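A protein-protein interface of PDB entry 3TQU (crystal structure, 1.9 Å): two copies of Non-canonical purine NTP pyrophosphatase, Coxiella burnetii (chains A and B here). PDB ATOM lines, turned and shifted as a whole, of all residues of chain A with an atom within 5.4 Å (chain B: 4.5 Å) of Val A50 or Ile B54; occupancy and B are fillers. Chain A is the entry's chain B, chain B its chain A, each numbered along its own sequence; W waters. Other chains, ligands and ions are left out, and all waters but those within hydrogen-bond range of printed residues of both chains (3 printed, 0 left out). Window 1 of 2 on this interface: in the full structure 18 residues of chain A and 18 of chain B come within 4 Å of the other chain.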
ATOM      1  N   THR A  48     -22.674  -3.498 -30.753  1.00  0.00           N
ATOM      2  CA  THR A  48     -21.446  -3.299 -29.985  1.00  0.00           C
ATOM      3  C   THR A  48     -20.884  -4.642 -29.531  1.00  0.00           C
ATOM      4  O   THR A  48     -21.628  -5.608 -29.361  1.00  0.00           O
ATOM      5  CB  THR A  48     -21.684  -2.413 -28.744  1.00  0.00           C
ATOM      6  OG1 THR A  48     -22.578  -3.078 -27.841  1.00  0.00           O
ATOM      7  CG2 THR A  48     -22.274  -1.064 -29.146  1.00  0.00           C
ATOM      8  N   PHE A  49     -19.568  -4.703 -29.339  1.00  0.00           N
ATOM      9  CA  PHE A  49     -18.931  -5.924 -28.863  1.00  0.00           C
ATOM     10  C   PHE A  49     -19.512  -6.350 -27.519  1.00  0.00           C
ATOM     11  O   PHE A  49     -19.752  -7.535 -27.282  1.00  0.00           O
ATOM     12  CB  PHE A  49     -17.416  -5.737 -28.733  1.00  0.00           C
ATOM     13  CG  PHE A  49     -16.752  -5.256 -29.990  1.00  0.00           C
ATOM     14  CD1 PHE A  49     -16.785  -6.021 -31.146  1.00  0.00           C
ATOM     15  CD2 PHE A  49     -16.082  -4.044 -30.014  1.00  0.00           C
ATOM     16  CE1 PHE A  49     -16.169  -5.581 -32.307  1.00  0.00           C
ATOM     17  CE2 PHE A  49     -15.462  -3.598 -31.170  1.00  0.00           C
ATOM     18  CZ  PHE A  49     -15.507  -4.370 -32.318  1.00  0.00           C
ATOM     19  N   VAL A  50     -19.740  -5.379 -26.640  1.00  0.00           N
ATOM     20  CA  VAL A  50     -20.245  -5.673 -25.307  1.00  0.00           C
ATOM     21  C   VAL A  50     -21.624  -6.324 -25.386  1.00  0.00           C
ATOM     22  O   VAL A  50     -21.885  -7.323 -24.715  1.00  0.00           O
ATOM     23  CB  VAL A  50     -20.272  -4.409 -24.403  1.00  0.00           C
ATOM     24  CG1 VAL A  50     -21.115  -3.320 -25.026  1.00  0.00           C
ATOM     25  CG2 VAL A  50     -20.771  -4.758 -23.006  1.00  0.00           C
ATOM     26  N   GLU A  51     -22.496  -5.776 -26.227  1.00  0.00           N
ATOM     27  CA  GLU A  51     -23.826  -6.354 -26.397  1.00  0.00           C
ATOM     28  C   GLU A  51     -23.753  -7.816 -26.834  1.00  0.00           C
ATOM     29  O   GLU A  51     -24.498  -8.656 -26.333  1.00  0.00           O
ATOM     30  CB  GLU A  51     -24.648  -5.553 -27.405  1.00  0.00           C
ATOM     31  CG  GLU A  51     -25.265  -4.278 -26.850  1.00  0.00           C
ATOM     32  CD  GLU A  51     -25.867  -3.416 -27.945  1.00  0.00           C
ATOM     33  OE1 GLU A  51     -25.152  -3.127 -28.924  1.00  0.00           O
ATOM     34  OE2 GLU A  51     -27.054  -3.039 -27.834  1.00  0.00           O
ATOM     35  N   ASN A  52     -22.858  -8.118 -27.768  1.00  0.00           N
ATOM     36  CA  ASN A  52     -22.708  -9.489 -28.260  1.00  0.00           C
ATOM     37  C   ASN A  52     -22.089 -10.433 -27.230  1.00  0.00           C
ATOM     38  O   ASN A  52     -22.487 -11.597 -27.123  1.00  0.00           O
ATOM     39  CB  ASN A  52     -21.897  -9.521 -29.559  1.00  0.00           C
ATOM     40  CG  ASN A  52     -22.667  -8.961 -30.736  1.00  0.00           C
ATOM     41  OD1 ASN A  52     -23.895  -9.010 -30.762  1.00  0.00           O
ATOM     42  ND2 ASN A  52     -21.950  -8.422 -31.714  1.00  0.00           N
ATOM     43  N   ALA A  53     -21.107  -9.935 -26.486  1.00  0.00           N
ATOM     44  CA  ALA A  53     -20.497 -10.717 -25.416  1.00  0.00           C
ATOM     45  C   ALA A  53     -21.561 -11.110 -24.394  1.00  0.00           C
ATOM     46  O   ALA A  53     -21.612 -12.248 -23.940  1.00  0.00           O
ATOM     47  CB  ALA A  53     -19.384  -9.927 -24.747  1.00  0.00           C
ATOM     48  N   ILE A  54     -22.414 -10.156 -24.040  1.00  0.00           N
ATOM     49  CA  ILE A  54     -23.486 -10.401 -23.079  1.00  0.00           C
ATOM     50  C   ILE A  54     -24.507 -11.401 -23.611  1.00  0.00           C
ATOM     51  O   ILE A  54     -24.928 -12.312 -22.895  1.00  0.00           O
ATOM     52  CB  ILE A  54     -24.192  -9.090 -22.694  1.00  0.00           C
ATOM     53  CG1 ILE A  54     -23.252  -8.221 -21.857  1.00  0.00           C
ATOM     54  CG2 ILE A  54     -25.477  -9.378 -21.926  1.00  0.00           C
ATOM     55  CD1 ILE A  54     -23.744  -6.809 -21.650  1.00  0.00           C
ATOM     56  N   ILE A  55     -24.911 -11.223 -24.864  1.00  0.00           N
ATOM     57  CA  ILE A  55     -25.816 -12.175 -25.501  1.00  0.00           C
ATOM     58  C   ILE A  55     -25.281 -13.600 -25.358  1.00  0.00           C
ATOM     59  O   ILE A  55     -25.979 -14.496 -24.884  1.00  0.00           O
ATOM     60  CB  ILE A  55     -26.029 -11.841 -26.992  1.00  0.00           C
ATOM     61  CG1 ILE A  55     -26.923 -10.606 -27.132  1.00  0.00           C
ATOM     62  CG2 ILE A  55     -26.641 -13.023 -27.722  1.00  0.00           C
ATOM     63  CD1 ILE A  55     -27.108 -10.138 -28.560  1.00  0.00           C
ATOM     64  N   ASP A  72     -16.551 -10.740 -27.344  1.00  0.00           N
ATOM     65  CA  ASP A  72     -16.696 -10.364 -28.736  1.00  0.00           C
ATOM     66  C   ASP A  72     -15.542  -9.438 -29.078  1.00  0.00           C
ATOM     67  O   ASP A  72     -15.104  -8.650 -28.239  1.00  0.00           O
ATOM     68  CB  ASP A  72     -18.037  -9.684 -29.017  1.00  0.00           C
ATOM     69  CG  ASP A  72     -18.313  -9.588 -30.497  1.00  0.00           C
ATOM     70  OD1 ASP A  72     -17.766 -10.445 -31.212  1.00  0.00           O
ATOM     71  OD2 ASP A  72     -19.034  -8.675 -30.953  1.00  0.00           O
ATOM     72  N   VAL A 124     -13.841  -7.377 -25.863  1.00  0.00           N
ATOM     73  CA  VAL A 124     -14.697  -7.161 -24.710  1.00  0.00           C
ATOM     74  C   VAL A 124     -15.120  -8.497 -24.127  1.00  0.00           C
ATOM     75  O   VAL A 124     -15.705  -9.331 -24.821  1.00  0.00           O
ATOM     76  CB  VAL A 124     -15.947  -6.345 -25.063  1.00  0.00           C
ATOM     77  CG1 VAL A 124     -16.828  -6.173 -23.827  1.00  0.00           C
ATOM     78  CG2 VAL A 124     -15.557  -4.991 -25.638  1.00  0.00           C
ATOM     79  N   ALA A 126     -17.271 -10.532 -21.081  1.00  0.00           N
ATOM     80  CA  ALA A 126     -18.377 -10.400 -20.144  1.00  0.00           C
ATOM     81  C   ALA A 126     -18.537 -11.673 -19.327  1.00  0.00           C
ATOM     82  O   ALA A 126     -18.607 -12.769 -19.881  1.00  0.00           O
ATOM     83  CB  ALA A 126     -19.667 -10.085 -20.881  1.00  0.00           C
ATOM     84  N   ILE A 138     -17.467  -6.561 -16.988  1.00  0.00           N
ATOM     85  CA  ILE A 138     -17.046  -6.224 -18.342  1.00  0.00           C
ATOM     86  C   ILE A 138     -15.573  -5.831 -18.350  1.00  0.00           C
ATOM     87  O   ILE A 138     -15.175  -4.883 -17.675  1.00  0.00           O
ATOM     88  CB  ILE A 138     -17.869  -5.050 -18.905  1.00  0.00           C
ATOM     89  CG1 ILE A 138     -19.363  -5.363 -18.836  1.00  0.00           C
ATOM     90  CG2 ILE A 138     -17.448  -4.726 -20.336  1.00  0.00           C
ATOM     91  CD1 ILE A 138     -19.776  -6.523 -19.691  1.00  0.00           C
ATOM     92  N   VAL B  50     -25.781  -2.128 -18.406  1.00  0.00           N
ATOM     93  CA  VAL B  50     -24.947  -1.739 -19.537  1.00  0.00           C
ATOM     94  C   VAL B  50     -25.743  -1.729 -20.843  1.00  0.00           C
ATOM     95  O   VAL B  50     -25.574  -0.837 -21.669  1.00  0.00           O
ATOM     96  CB  VAL B  50     -23.692  -2.628 -19.667  1.00  0.00           C
ATOM     97  CG1 VAL B  50     -24.084  -4.079 -19.854  1.00  0.00           C
ATOM     98  CG2 VAL B  50     -22.823  -2.150 -20.814  1.00  0.00           C
ATOM     99  N   GLU B  51     -26.624  -2.708 -21.021  1.00  0.00           N
ATOM    100  CA  GLU B  51     -27.474  -2.748 -22.210  1.00  0.00           C
ATOM    101  C   GLU B  51     -28.394  -1.529 -22.314  1.00  0.00           C
ATOM    102  O   GLU B  51     -28.589  -0.975 -23.397  1.00  0.00           O
ATOM    103  CB  GLU B  51     -28.296  -4.040 -22.250  1.00  0.00           C
ATOM    104  CG  GLU B  51     -27.491  -5.253 -22.705  1.00  0.00           C
ATOM    105  CD  GLU B  51     -28.244  -6.553 -22.532  1.00  0.00           C
ATOM    106  OE1 GLU B  51     -28.654  -6.848 -21.393  1.00  0.00           O
ATOM    107  OE2 GLU B  51     -28.429  -7.279 -23.532  1.00  0.00           O
ATOM    108  N   ASN B  52     -28.964  -1.118 -21.190  1.00  0.00           N
ATOM    109  CA  ASN B  52     -29.846   0.041 -21.180  1.00  0.00           C
ATOM    110  C   ASN B  52     -29.072   1.337 -21.400  1.00  0.00           C
ATOM    111  O   ASN B  52     -29.525   2.231 -22.118  1.00  0.00           O
ATOM    112  CB  ASN B  52     -30.654   0.094 -19.882  1.00  0.00           C
ATOM    113  CG  ASN B  52     -31.742  -0.964 -19.835  1.00  0.00           C
ATOM    114  OD1 ASN B  52     -32.338  -1.303 -20.859  1.00  0.00           O
ATOM    115  ND2 ASN B  52     -32.005  -1.494 -18.644  1.00  0.00           N
ATOM    116  N   ALA B  53     -27.894   1.424 -20.789  1.00  0.00           N
ATOM    117  CA  ALA B  53     -27.027   2.580 -20.967  1.00  0.00           C
ATOM    118  C   ALA B  53     -26.692   2.764 -22.441  1.00  0.00           C
ATOM    119  O   ALA B  53     -26.734   3.878 -22.965  1.00  0.00           O
ATOM    120  CB  ALA B  53     -25.751   2.427 -20.141  1.00  0.00           C
ATOM    121  N   ILE B  54     -26.371   1.664 -23.116  1.00  0.00           N
ATOM    122  CA  ILE B  54     -26.054   1.722 -24.541  1.00  0.00           C
ATOM    123  C   ILE B  54     -27.279   2.084 -25.372  1.00  0.00           C
ATOM    124  O   ILE B  54     -27.202   2.923 -26.272  1.00  0.00           O
ATOM    125  CB  ILE B  54     -25.446   0.397 -25.042  1.00  0.00           C
ATOM    126  CG1 ILE B  54     -24.025   0.245 -24.496  1.00  0.00           C
ATOM    127  CG2 ILE B  54     -25.428   0.363 -26.554  1.00  0.00           C
ATOM    128  CD1 ILE B  54     -23.447  -1.135 -24.666  1.00  0.00           C
ATOM    129  N   ILE B  55     -28.407   1.451 -25.064  1.00  0.00           N
ATOM    130  CA  ILE B  55     -29.649   1.710 -25.782  1.00  0.00           C
ATOM    131  C   ILE B  55     -29.966   3.202 -25.795  1.00  0.00           C
ATOM    132  O   ILE B  55     -30.338   3.758 -26.824  1.00  0.00           O
ATOM    133  CB  ILE B  55     -30.834   0.935 -25.169  1.00  0.00           C
ATOM    134  CG1 ILE B  55     -30.745  -0.552 -25.534  1.00  0.00           C
ATOM    135  CG2 ILE B  55     -32.159   1.517 -25.645  1.00  0.00           C
ATOM    136  CD1 ILE B  55     -31.826  -1.408 -24.893  1.00  0.00           C
ATOM    137  N   LYS B  56     -29.797   3.846 -24.645  1.00  0.00           N
ATOM    138  CA  LYS B  56     -30.171   5.246 -24.497  1.00  0.00           C
ATOM    139  C   LYS B  56     -29.140   6.189 -25.119  1.00  0.00           C
ATOM    140  O   LYS B  56     -29.499   7.205 -25.714  1.00  0.00           O
ATOM    141  CB  LYS B  56     -30.415   5.579 -23.023  1.00  0.00           C
ATOM    142  CG  LYS B  56     -31.552   4.766 -22.406  1.00  0.00           C
ATOM    143  CD  LYS B  56     -31.906   5.245 -21.009  1.00  0.00           C
ATOM    144  CE  LYS B  56     -30.744   5.072 -20.043  1.00  0.00           C
ATOM    145  NZ  LYS B  56     -31.144   5.425 -18.647  1.00  0.00           N
ATOM    146  N   ALA B  57     -27.863   5.847 -24.993  1.00  0.00           N
ATOM    147  CA  ALA B  57     -26.810   6.654 -25.597  1.00  0.00           C
ATOM    148  C   ALA B  57     -26.841   6.559 -27.123  1.00  0.00           C
ATOM    149  O   ALA B  57     -26.698   7.565 -27.817  1.00  0.00           O
ATOM    150  CB  ALA B  57     -25.442   6.247 -25.056  1.00  0.00           C
ATOM    151  N   ARG B  58     -27.030   5.352 -27.644  1.00  0.00           N
ATOM    152  CA  ARG B  58     -27.085   5.164 -29.089  1.00  0.00           C
ATOM    153  C   ARG B  58     -28.254   5.927 -29.695  1.00  0.00           C
ATOM    154  O   ARG B  58     -28.139   6.497 -30.781  1.00  0.00           O
ATOM    155  CB  ARG B  58     -27.196   3.686 -29.460  1.00  0.00           C
ATOM    156  CG  ARG B  58     -27.249   3.470 -30.967  1.00  0.00           C
ATOM    157  CD  ARG B  58     -27.905   2.155 -31.349  1.00  0.00           C
ATOM    158  NE  ARG B  58     -27.157   0.991 -30.887  1.00  0.00           N
ATOM    159  CZ  ARG B  58     -27.613   0.132 -29.984  1.00  0.00           C
ATOM    160  NH1 ARG B  58     -28.809   0.312 -29.447  1.00  0.00           N
ATOM    161  NH2 ARG B  58     -26.878  -0.903 -29.616  1.00  0.00           N
ATOM    162  N   ALA B 126     -22.360   4.785 -20.362  1.00  0.00           N
ATOM    163  CA  ALA B 126     -21.894   4.485 -21.707  1.00  0.00           C
ATOM    164  C   ALA B 126     -21.725   5.779 -22.485  1.00  0.00           C
ATOM    165  O   ALA B 126     -22.624   6.617 -22.510  1.00  0.00           O
ATOM    166  CB  ALA B 126     -22.863   3.549 -22.421  1.00  0.00           C
ATOM    167  N   PRO B 136     -18.169   1.551 -27.278  1.00  0.00           N
ATOM    168  CA  PRO B 136     -18.395   2.706 -26.409  1.00  0.00           C
ATOM    169  C   PRO B 136     -17.544   2.608 -25.152  1.00  0.00           C
ATOM    170  O   PRO B 136     -17.203   1.505 -24.720  1.00  0.00           O
ATOM    171  CB  PRO B 136     -19.880   2.583 -26.045  1.00  0.00           C
ATOM    172  CG  PRO B 136     -20.191   1.132 -26.210  1.00  0.00           C
ATOM    173  CD  PRO B 136     -19.364   0.694 -27.380  1.00  0.00           C
ATOM    174  N   ILE B 138     -17.205   2.306 -21.460  1.00  0.00           N
ATOM    175  CA  ILE B 138     -18.090   1.814 -20.412  1.00  0.00           C
ATOM    176  C   ILE B 138     -17.447   2.040 -19.050  1.00  0.00           C
ATOM    177  O   ILE B 138     -16.348   1.552 -18.790  1.00  0.00           O
ATOM    178  CB  ILE B 138     -18.387   0.310 -20.575  1.00  0.00           C
ATOM    179  CG1 ILE B 138     -18.985   0.023 -21.958  1.00  0.00           C
ATOM    180  CG2 ILE B 138     -19.310  -0.179 -19.464  1.00  0.00           C
ATOM    181  CD1 ILE B 138     -20.299   0.728 -22.221  1.00  0.00           C
HETATM  182  O   HOH W   1     -26.908  -7.378 -25.711  1.00  0.00           O
HETATM  183  O   HOH W   2     -28.341  -3.026 -25.352  1.00  0.00           O
HETATM  184  O   HOH W   3     -28.107  -3.948 -30.347  1.00  0.00           O
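Thr A48 touches Ile B54.
CG2 of Thr A48 touches CD of Pro B136, 3.8 Å away.
CG2 of Val A50 touches CG2 of Val B50, 3.98 Å away.
Ile B54 touches Val A50.
CG2 of Ile B54 touches OE2 of Glu A51, 3.98 Å away.
CG1 of Val B50 touches CD1 of Ile A54, 3.3 Å away.
CG2 of Ile A54 touches OE2 of Glu B51, at 3.96 Å.
Water W1 bridges OE2 of Glu B51 (2.7 Å) and O of Glu A51 (2.8 Å).
Water W2 lies within hydrogen-bond range of the side-chain carboxylate of Glu A51 (2.8 Å) and the backbone carbonyl oxygen of Glu B51 (2.8 Å).
Water W3 bridges the side-chain carboxylate of Glu A51 (2.9 Å) and the guanidinium group of Arg B58 (3.4 Å).
Val A50 touches its own counterpart, Val B50.
Val A50 touches Ile B54, and with the chains exchanged Ile A54 touches Val B50.
Glu A51 touches Ile B54, and with the chains exchanged Ile A54 touches Glu B51.
Positions printed for both chains: 50, 51, 52, 53, 54, 55, 126 and 138.
Of the 8 pairs that touch across the chains among the printed residues, 5 have their exchanged pair printed and touching as well.
The side-chain hydroxyl (OG1) of Thr A48 is in hydrogen-bond range of the side-chain carboxylate (OE1) of Glu A51 (2.8 Å).
Of the 12 printed residues of chain A, 4 touch a printed residue of chain B.
Along chain A the printed residues that touch a printed residue of chain B span positions 48 to 54.
Hydrophobic or aromatic side chains of chain B within 4 Å of the printed part of chain A: Val B50, Ile B54 and Pro B136.
Along chain B the printed residues that touch a printed residue of chain A span positions 50 to 136.
Among the printed residues, Asp or Glu carboxylates within 4 Å of a Lys or Arg side-chain nitrogen of the other chain: Glu A51 with Arg B58.
Printed residues of chain B within 4 Å of Thr A48: Ile B54 and Pro B136.
Val A50 touches two residues of chain B.
Printed residues of chain B within 4 Å of Glu A51: Ile B54 (3.98 Å) and Arg B58 (2.8 Å).
Printed residues of chain B within 4 Å of Ile A54: Val B50 (3.3 Å) and Glu B51 (3.96 Å).
Of the printed residues of chain A, Val B50 touches Val A50 (3.98 Å) and Ile A54 (3.3 Å).
Of the printed residues of chain A, Ile B54 touches Thr A48, Val A50 and Glu A51.
Of the printed residues of chain A, Arg B58 touches Glu A51 (2.8 Å).
The nearest printed residue of chain B that does not touch Val A50 is Pro B136 (4.7 Å).
The guanidinium group of Arg B58 is in salt-bridge range of the side-chain carboxylate of Glu A51, at 2.8 Å.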
